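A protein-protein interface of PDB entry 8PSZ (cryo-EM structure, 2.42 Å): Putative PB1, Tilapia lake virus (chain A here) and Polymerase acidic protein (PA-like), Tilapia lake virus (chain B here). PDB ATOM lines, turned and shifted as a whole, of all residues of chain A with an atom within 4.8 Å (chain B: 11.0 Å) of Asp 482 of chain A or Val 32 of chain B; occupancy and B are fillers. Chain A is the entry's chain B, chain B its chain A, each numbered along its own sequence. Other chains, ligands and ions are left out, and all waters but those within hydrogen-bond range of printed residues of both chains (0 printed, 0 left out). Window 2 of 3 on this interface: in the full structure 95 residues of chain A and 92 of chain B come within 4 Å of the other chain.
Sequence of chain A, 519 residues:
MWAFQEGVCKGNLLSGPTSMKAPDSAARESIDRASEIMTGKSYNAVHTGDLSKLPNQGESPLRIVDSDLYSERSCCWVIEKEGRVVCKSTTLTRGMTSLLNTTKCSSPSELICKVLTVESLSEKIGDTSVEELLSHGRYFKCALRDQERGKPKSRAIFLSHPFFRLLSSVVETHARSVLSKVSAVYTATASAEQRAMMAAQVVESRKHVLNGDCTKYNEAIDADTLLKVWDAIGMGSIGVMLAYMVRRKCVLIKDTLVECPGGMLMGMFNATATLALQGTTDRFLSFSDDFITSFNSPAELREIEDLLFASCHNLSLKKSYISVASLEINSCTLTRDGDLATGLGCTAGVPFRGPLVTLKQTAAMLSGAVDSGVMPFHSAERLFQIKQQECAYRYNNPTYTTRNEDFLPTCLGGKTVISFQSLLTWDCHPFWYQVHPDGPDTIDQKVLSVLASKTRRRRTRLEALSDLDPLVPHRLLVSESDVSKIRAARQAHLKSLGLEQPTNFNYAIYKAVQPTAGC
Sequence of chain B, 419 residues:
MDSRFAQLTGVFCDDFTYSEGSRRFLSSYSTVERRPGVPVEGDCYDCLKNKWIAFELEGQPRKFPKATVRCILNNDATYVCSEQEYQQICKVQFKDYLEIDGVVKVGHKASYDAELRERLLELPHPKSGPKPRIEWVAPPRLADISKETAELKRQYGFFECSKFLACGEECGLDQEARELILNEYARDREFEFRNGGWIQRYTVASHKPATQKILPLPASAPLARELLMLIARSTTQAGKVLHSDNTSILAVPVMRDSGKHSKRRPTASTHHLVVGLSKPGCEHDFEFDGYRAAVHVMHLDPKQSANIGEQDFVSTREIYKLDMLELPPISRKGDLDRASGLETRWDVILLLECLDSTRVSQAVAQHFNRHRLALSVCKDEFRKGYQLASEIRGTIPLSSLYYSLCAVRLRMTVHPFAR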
ATOM      1  N   LEU A 477     -26.881  19.334  11.159  1.00  0.00           N
ATOM      2  CA  LEU A 477     -28.193  19.931  11.352  1.00  0.00           C
ATOM      3  C   LEU A 477     -28.235  20.764  12.627  1.00  0.00           C
ATOM      4  O   LEU A 477     -27.522  20.493  13.596  1.00  0.00           O
ATOM      5  CB  LEU A 477     -29.268  18.845  11.412  1.00  0.00           C
ATOM      6  CG  LEU A 477     -29.373  17.938  10.187  1.00  0.00           C
ATOM      7  CD1 LEU A 477     -30.406  16.850  10.422  1.00  0.00           C
ATOM      8  CD2 LEU A 477     -29.713  18.745   8.945  1.00  0.00           C
ATOM      9  N   VAL A 478     -29.083  21.790  12.612  1.00  0.00           N
ATOM     10  CA  VAL A 478     -29.302  22.653  13.767  1.00  0.00           C
ATOM     11  C   VAL A 478     -30.780  23.004  13.840  1.00  0.00           C
ATOM     12  O   VAL A 478     -31.422  23.254  12.815  1.00  0.00           O
ATOM     13  CB  VAL A 478     -28.452  23.939  13.699  1.00  0.00           C
ATOM     14  CG1 VAL A 478     -26.975  23.601  13.642  1.00  0.00           C
ATOM     15  CG2 VAL A 478     -28.862  24.791  12.504  1.00  0.00           C
ATOM     16  N   SER A 479     -31.318  23.020  15.055  1.00  0.00           N
ATOM     17  CA  SER A 479     -32.645  23.546  15.317  1.00  0.00           C
ATOM     18  C   SER A 479     -32.521  24.967  15.860  1.00  0.00           C
ATOM     19  O   SER A 479     -31.424  25.491  16.061  1.00  0.00           O
ATOM     20  CB  SER A 479     -33.400  22.641  16.291  1.00  0.00           C
ATOM     21  OG  SER A 479     -32.631  22.386  17.452  1.00  0.00           O
ATOM     22  N   GLU A 480     -33.668  25.606  16.093  1.00  0.00           N
ATOM     23  CA  GLU A 480     -33.656  26.949  16.663  1.00  0.00           C
ATOM     24  C   GLU A 480     -32.997  26.948  18.038  1.00  0.00           C
ATOM     25  O   GLU A 480     -32.145  27.797  18.340  1.00  0.00           O
ATOM     26  CB  GLU A 480     -35.085  27.486  16.744  1.00  0.00           C
ATOM     27  CG  GLU A 480     -35.172  28.980  16.983  1.00  0.00           C
ATOM     28  CD  GLU A 480     -36.572  29.429  17.344  1.00  0.00           C
ATOM     29  OE1 GLU A 480     -37.539  28.878  16.779  1.00  0.00           O
ATOM     30  OE2 GLU A 480     -36.705  30.335  18.194  1.00  0.00           O
ATOM     31  N   SER A 481     -33.370  25.984  18.882  1.00  0.00           N
ATOM     32  CA  SER A 481     -32.754  25.877  20.198  1.00  0.00           C
ATOM     33  C   SER A 481     -31.267  25.577  20.079  1.00  0.00           C
ATOM     34  O   SER A 481     -30.466  26.057  20.886  1.00  0.00           O
ATOM     35  CB  SER A 481     -33.456  24.797  21.023  1.00  0.00           C
ATOM     36  OG  SER A 481     -32.817  23.542  20.872  1.00  0.00           O
ATOM     37  N   ASP A 482     -30.878  24.779  19.081  1.00  0.00           N
ATOM     38  CA  ASP A 482     -29.459  24.522  18.859  1.00  0.00           C
ATOM     39  C   ASP A 482     -28.715  25.809  18.530  1.00  0.00           C
ATOM     40  O   ASP A 482     -27.613  26.042  19.037  1.00  0.00           O
ATOM     41  CB  ASP A 482     -29.273  23.506  17.734  1.00  0.00           C
ATOM     42  CG  ASP A 482     -29.843  22.147  18.076  1.00  0.00           C
ATOM     43  OD1 ASP A 482     -30.824  22.086  18.845  1.00  0.00           O
ATOM     44  OD2 ASP A 482     -29.310  21.138  17.568  1.00  0.00           O
ATOM     45  N   VAL A 483     -29.295  26.650  17.673  1.00  0.00           N
ATOM     46  CA  VAL A 483     -28.649  27.914  17.327  1.00  0.00           C
ATOM     47  C   VAL A 483     -28.503  28.784  18.568  1.00  0.00           C
ATOM     48  O   VAL A 483     -27.440  29.365  18.823  1.00  0.00           O
ATOM     49  CB  VAL A 483     -29.444  28.637  16.222  1.00  0.00           C
ATOM     50  CG1 VAL A 483     -28.957  30.070  16.061  1.00  0.00           C
ATOM     51  CG2 VAL A 483     -29.333  27.884  14.907  1.00  0.00           C
ATOM     52  N   SER A 484     -29.571  28.874  19.365  1.00  0.00           N
ATOM     53  CA  SER A 484     -29.509  29.679  20.581  1.00  0.00           C
ATOM     54  C   SER A 484     -28.438  29.158  21.532  1.00  0.00           C
ATOM     55  O   SER A 484     -27.657  29.939  22.089  1.00  0.00           O
ATOM     56  CB  SER A 484     -30.873  29.693  21.268  1.00  0.00           C
ATOM     57  OG  SER A 484     -31.626  30.830  20.882  1.00  0.00           O
ATOM     58  N   LYS A 485     -28.383  27.838  21.724  1.00  0.00           N
ATOM     59  CA  LYS A 485     -27.414  27.256  22.646  1.00  0.00           C
ATOM     60  C   LYS A 485     -25.989  27.472  22.160  1.00  0.00           C
ATOM     61  O   LYS A 485     -25.096  27.788  22.955  1.00  0.00           O
ATOM     62  CB  LYS A 485     -27.694  25.763  22.818  1.00  0.00           C
ATOM     63  CG  LYS A 485     -28.471  25.423  24.075  1.00  0.00           C
ATOM     64  CD  LYS A 485     -29.013  24.005  24.030  1.00  0.00           C
ATOM     65  CE  LYS A 485     -30.373  23.906  24.699  1.00  0.00           C
ATOM     66  NZ  LYS A 485     -31.431  24.622  23.936  1.00  0.00           N
ATOM     67  N   ILE A 486     -25.750  27.293  20.860  1.00  0.00           N
ATOM     68  CA  ILE A 486     -24.408  27.481  20.320  1.00  0.00           C
ATOM     69  C   ILE A 486     -23.971  28.929  20.488  1.00  0.00           C
ATOM     70  O   ILE A 486     -22.834  29.208  20.894  1.00  0.00           O
ATOM     71  CB  ILE A 486     -24.362  27.041  18.845  1.00  0.00           C
ATOM     72  CG1 ILE A 486     -24.665  25.548  18.722  1.00  0.00           C
ATOM     73  CG2 ILE A 486     -23.002  27.345  18.240  1.00  0.00           C
ATOM     74  CD1 ILE A 486     -25.230  25.152  17.375  1.00  0.00           C
ATOM     75  N   MET B   1     -15.924   9.999   9.498  1.00  0.00           N
ATOM     76  CA  MET B   1     -17.230  10.645   9.821  1.00  0.00           C
ATOM     77  C   MET B   1     -18.216  10.499   8.666  1.00  0.00           C
ATOM     78  O   MET B   1     -17.960  10.963   7.556  1.00  0.00           O
ATOM     79  CB  MET B   1     -17.029  12.126  10.147  1.00  0.00           C
ATOM     80  CG  MET B   1     -17.844  12.606  11.332  1.00  0.00           C
ATOM     81  SD  MET B   1     -17.377  14.253  11.894  1.00  0.00           S
ATOM     82  CE  MET B   1     -18.989  14.948  12.247  1.00  0.00           C
ATOM     83  N   GLY B  10     -26.752   9.110  18.150  1.00  0.00           N
ATOM     84  CA  GLY B  10     -27.655   9.733  19.102  1.00  0.00           C
ATOM     85  C   GLY B  10     -28.272   8.729  20.053  1.00  0.00           C
ATOM     86  O   GLY B  10     -28.481   9.024  21.233  1.00  0.00           O
ATOM     87  N   CYS B  13     -25.789   7.847  22.986  1.00  0.00           N
ATOM     88  CA  CYS B  13     -25.805   8.855  24.047  1.00  0.00           C
ATOM     89  C   CYS B  13     -27.260   9.163  24.369  1.00  0.00           C
ATOM     90  O   CYS B  13     -27.870  10.071  23.802  1.00  0.00           O
ATOM     91  CB  CYS B  13     -25.044  10.106  23.624  1.00  0.00           C
ATOM     92  SG  CYS B  13     -23.818   9.855  22.317  1.00  0.00           S
ATOM     93  N   ARG B  23     -23.166  15.625  30.809  1.00  0.00           N
ATOM     94  CA  ARG B  23     -23.383  14.586  29.811  1.00  0.00           C
ATOM     95  C   ARG B  23     -22.104  13.786  29.602  1.00  0.00           C
ATOM     96  O   ARG B  23     -21.007  14.346  29.523  1.00  0.00           O
ATOM     97  CB  ARG B  23     -23.836  15.209  28.490  1.00  0.00           C
ATOM     98  CG  ARG B  23     -25.015  14.509  27.835  1.00  0.00           C
ATOM     99  CD  ARG B  23     -25.648  15.388  26.767  1.00  0.00           C
ATOM    100  NE  ARG B  23     -26.647  14.675  25.980  1.00  0.00           N
ATOM    101  CZ  ARG B  23     -26.369  13.741  25.080  1.00  0.00           C
ATOM    102  NH1 ARG B  23     -25.123  13.373  24.826  1.00  0.00           N
ATOM    103  NH2 ARG B  23     -27.365  13.161  24.418  1.00  0.00           N
ATOM    104  N   PHE B  25     -21.499  11.021  27.043  1.00  0.00           N
ATOM    105  CA  PHE B  25     -21.152  10.780  25.649  1.00  0.00           C
ATOM    106  C   PHE B  25     -21.577  11.967  24.794  1.00  0.00           C
ATOM    107  O   PHE B  25     -22.744  12.367  24.813  1.00  0.00           O
ATOM    108  CB  PHE B  25     -21.812   9.499  25.137  1.00  0.00           C
ATOM    109  CG  PHE B  25     -21.283   8.248  25.775  1.00  0.00           C
ATOM    110  CD1 PHE B  25     -19.974   7.849  25.570  1.00  0.00           C
ATOM    111  CD2 PHE B  25     -22.098   7.468  26.579  1.00  0.00           C
ATOM    112  CE1 PHE B  25     -19.489   6.697  26.157  1.00  0.00           C
ATOM    113  CE2 PHE B  25     -21.616   6.316  27.166  1.00  0.00           C
ATOM    114  CZ  PHE B  25     -20.310   5.930  26.953  1.00  0.00           C
ATOM    115  N   LEU B  26     -20.626  12.519  24.044  1.00  0.00           N
ATOM    116  CA  LEU B  26     -20.854  13.672  23.182  1.00  0.00           C
ATOM    117  C   LEU B  26     -20.795  13.218  21.731  1.00  0.00           C
ATOM    118  O   LEU B  26     -19.788  12.650  21.298  1.00  0.00           O
ATOM    119  CB  LEU B  26     -19.814  14.762  23.443  1.00  0.00           C
ATOM    120  CG  LEU B  26     -19.738  15.284  24.877  1.00  0.00           C
ATOM    121  CD1 LEU B  26     -18.577  16.252  25.022  1.00  0.00           C
ATOM    122  CD2 LEU B  26     -21.045  15.943  25.283  1.00  0.00           C
ATOM    123  N   SER B  27     -21.864  13.476  20.982  1.00  0.00           N
ATOM    124  CA  SER B  27     -21.947  13.031  19.598  1.00  0.00           C
ATOM    125  C   SER B  27     -21.229  14.014  18.681  1.00  0.00           C
ATOM    126  O   SER B  27     -21.434  15.227  18.773  1.00  0.00           O
ATOM    127  CB  SER B  27     -23.408  12.886  19.174  1.00  0.00           C
ATOM    128  OG  SER B  27     -23.508  12.542  17.805  1.00  0.00           O
ATOM    129  N   SER B  28     -20.386  13.482  17.791  1.00  0.00           N
ATOM    130  CA  SER B  28     -19.680  14.336  16.842  1.00  0.00           C
ATOM    131  C   SER B  28     -20.634  14.966  15.837  1.00  0.00           C
ATOM    132  O   SER B  28     -20.337  16.035  15.291  1.00  0.00           O
ATOM    133  CB  SER B  28     -18.606  13.533  16.112  1.00  0.00           C
ATOM    134  OG  SER B  28     -17.482  13.305  16.943  1.00  0.00           O
ATOM    135  N   TYR B  29     -21.772  14.326  15.578  1.00  0.00           N
ATOM    136  CA  TYR B  29     -22.742  14.845  14.624  1.00  0.00           C
ATOM    137  C   TYR B  29     -23.671  15.887  15.229  1.00  0.00           C
ATOM    138  O   TYR B  29     -24.387  16.558  14.483  1.00  0.00           O
ATOM    139  CB  TYR B  29     -23.569  13.697  14.047  1.00  0.00           C
ATOM    140  CG  TYR B  29     -22.725  12.584  13.476  1.00  0.00           C
ATOM    141  CD1 TYR B  29     -22.313  11.523  14.270  1.00  0.00           C
ATOM    142  CD2 TYR B  29     -22.331  12.598  12.147  1.00  0.00           C
ATOM    143  CE1 TYR B  29     -21.540  10.507  13.756  1.00  0.00           C
ATOM    144  CE2 TYR B  29     -21.556  11.587  11.624  1.00  0.00           C
ATOM    145  CZ  TYR B  29     -21.164  10.543  12.432  1.00  0.00           C
ATOM    146  OH  TYR B  29     -20.392   9.530  11.917  1.00  0.00           O
ATOM    147  N   SER B  30     -23.671  16.043  16.549  1.00  0.00           N
ATOM    148  CA  SER B  30     -24.527  17.015  17.215  1.00  0.00           C
ATOM    149  C   SER B  30     -23.791  18.345  17.302  1.00  0.00           C
ATOM    150  O   SER B  30     -22.671  18.409  17.819  1.00  0.00           O
ATOM    151  CB  SER B  30     -24.924  16.523  18.605  1.00  0.00           C
ATOM    152  OG  SER B  30     -25.556  17.551  19.347  1.00  0.00           O
ATOM    153  N   THR B  31     -24.421  19.404  16.793  1.00  0.00           N
ATOM    154  CA  THR B  31     -23.795  20.719  16.800  1.00  0.00           C
ATOM    155  C   THR B  31     -23.708  21.311  18.200  1.00  0.00           C
ATOM    156  O   THR B  31     -22.829  22.141  18.453  1.00  0.00           O
ATOM    157  CB  THR B  31     -24.567  21.672  15.887  1.00  0.00           C
ATOM    158  OG1 THR B  31     -25.950  21.301  15.864  1.00  0.00           O
ATOM    159  CG2 THR B  31     -24.009  21.628  14.474  1.00  0.00           C
ATOM    160  N   VAL B  32     -24.589  20.906  19.110  1.00  0.00           N
ATOM    161  CA  VAL B  32     -24.575  21.444  20.466  1.00  0.00           C
ATOM    162  C   VAL B  32     -23.637  20.653  21.370  1.00  0.00           C
ATOM    163  O   VAL B  32     -22.933  21.233  22.199  1.00  0.00           O
ATOM    164  CB  VAL B  32     -26.009  21.482  21.039  1.00  0.00           C
ATOM    165  CG1 VAL B  32     -26.853  22.494  20.281  1.00  0.00           C
ATOM    166  CG2 VAL B  32     -26.660  20.106  21.000  1.00  0.00           C
ATOM    167  N   GLU B  33     -23.606  19.326  21.225  1.00  0.00           N
ATOM    168  CA  GLU B  33     -22.757  18.492  22.068  1.00  0.00           C
ATOM    169  C   GLU B  33     -21.296  18.517  21.642  1.00  0.00           C
ATOM    170  O   GLU B  33     -20.429  18.148  22.439  1.00  0.00           O
ATOM    171  CB  GLU B  33     -23.262  17.049  22.058  1.00  0.00           C
ATOM    172  CG  GLU B  33     -24.636  16.872  22.676  1.00  0.00           C
ATOM    173  CD  GLU B  33     -25.301  15.578  22.249  1.00  0.00           C
ATOM    174  OE1 GLU B  33     -24.593  14.558  22.122  1.00  0.00           O
ATOM    175  OE2 GLU B  33     -26.532  15.583  22.040  1.00  0.00           O
ATOM    176  N   ARG B  34     -21.006  18.936  20.414  1.00  0.00           N
ATOM    177  CA  ARG B  34     -19.625  19.028  19.964  1.00  0.00           C
ATOM    178  C   ARG B  34     -18.834  19.969  20.862  1.00  0.00           C
ATOM    179  O   ARG B  34     -19.322  21.030  21.261  1.00  0.00           O
ATOM    180  CB  ARG B  34     -19.571  19.530  18.522  1.00  0.00           C
ATOM    181  CG  ARG B  34     -19.408  18.446  17.480  1.00  0.00           C
ATOM    182  CD  ARG B  34     -19.481  19.037  16.084  1.00  0.00           C
ATOM    183  NE  ARG B  34     -18.160  19.338  15.546  1.00  0.00           N
ATOM    184  CZ  ARG B  34     -17.486  18.559  14.710  1.00  0.00           C
ATOM    185  NH1 ARG B  34     -17.977  17.406  14.286  1.00  0.00           N
ATOM    186  NH2 ARG B  34     -16.289  18.950  14.283  1.00  0.00           N
ATOM    187  N   ARG B  35     -17.602  19.578  21.177  1.00  0.00           N
ATOM    188  CA  ARG B  35     -16.704  20.462  21.907  1.00  0.00           C
ATOM    189  C   ARG B  35     -16.035  21.401  20.910  1.00  0.00           C
ATOM    190  O   ARG B  35     -15.235  20.946  20.082  1.00  0.00           O
ATOM    191  CB  ARG B  35     -15.646  19.667  22.671  1.00  0.00           C
ATOM    192  CG  ARG B  35     -16.105  19.137  24.019  1.00  0.00           C
ATOM    193  CD  ARG B  35     -15.215  18.005  24.513  1.00  0.00           C
ATOM    194  NE  ARG B  35     -15.061  16.946  23.520  1.00  0.00           N
ATOM    195  CZ  ARG B  35     -13.933  16.292  23.276  1.00  0.00           C
ATOM    196  NH1 ARG B  35     -12.821  16.545  23.950  1.00  0.00           N
ATOM    197  NH2 ARG B  35     -13.918  15.355  22.333  1.00  0.00           N
ATOM    198  N   PRO B  36     -16.323  22.702  20.946  1.00  0.00           N
ATOM    199  CA  PRO B  36     -15.701  23.607  19.973  1.00  0.00           C
ATOM    200  C   PRO B  36     -14.188  23.638  20.132  1.00  0.00           C
ATOM    201  O   PRO B  36     -13.658  23.577  21.243  1.00  0.00           O
ATOM    202  CB  PRO B  36     -16.335  24.967  20.288  1.00  0.00           C
ATOM    203  CG  PRO B  36     -16.880  24.843  21.662  1.00  0.00           C
ATOM    204  CD  PRO B  36     -17.244  23.410  21.850  1.00  0.00           C
ATOM    205  N   GLY B  37     -13.494  23.732  19.001  1.00  0.00           N
ATOM    206  CA  GLY B  37     -12.048  23.807  19.021  1.00  0.00           C
ATOM    207  C   GLY B  37     -11.345  22.508  19.332  1.00  0.00           C
ATOM    208  O   GLY B  37     -10.177  22.532  19.726  1.00  0.00           O
ATOM    209  N   CYS B  47     -16.377  11.344  27.806  1.00  0.00           N
ATOM    210  CA  CYS B  47     -15.640  12.296  28.631  1.00  0.00           C
ATOM    211  C   CYS B  47     -15.110  11.641  29.899  1.00  0.00           C
ATOM    212  O   CYS B  47     -14.000  11.952  30.346  1.00  0.00           O
ATOM    213  CB  CYS B  47     -16.535  13.485  28.981  1.00  0.00           C
ATOM    214  SG  CYS B  47     -17.300  14.288  27.557  1.00  0.00           S
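The side-chain hydroxyl of Ser 479 of chain A lies close to the backbone NH of Asp 482 of chain A, at 3.4 Å. The side-chain hydroxyl of Ser 481 of chain A sits at hydrogen-bond distance from the side-chain carboxylate of Asp 482 of chain A.
Of the 18 printed residues of chain B, 2 touch a printed residue of chain A. Hydrophobic or aromatic side chains of chain B that line the printed part of chain A: Val 32.
The side-chain hydroxyl (OG1) of Thr 31 of chain B is in hydrogen-bond range of the backbone carbonyl oxygen (O) of Leu 477 of chain A.
Thr 31 of chain B touches Val 478 of chain A (OG1 to CG1, 3.4 Å). OD2 of Asp 482 of chain A touches OG1 of Thr 31 of chain B, at 3.8 Å. Asp 482 of chain A touches Val 32 of chain B. CD1 of Ile 486 of chain A touches CB of Thr 31 of chain B, 3.8 Å away.
Of the printed residues of chain B, Leu 477 of chain A touches Thr 31 (2.9 Å). No residue of chain B comes within 4 Å of Ser 479 of chain A. No residue of chain B comes within 4 Å of Ser 481 of chain A. Of chain B, only Thr 31 (3.8 Å) and Val 32 (3.6 Å) come within 4 Å of Asp 482 of chain A. Ser 484 of chain A touches none of the printed residues of chain B. No residue of chain B comes within 4 Å of Lys 485 of chain A. Of the printed residues of chain B, Ile 486 of chain A touches Thr 31 (3.8 Å). Printed residues of chain A within 4 Å of Thr 31 of chain B: Leu 477 (2.9 Å), Val 478 (3.4 Å), Asp 482 (3.8 Å) and Ile 486 (3.8 Å). Of chain A, only Asp 482 (3.6 Å) comes within 4 Å of Val 32 of chain B. Cys 47 of chain B touches none of the printed residues of chain A.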
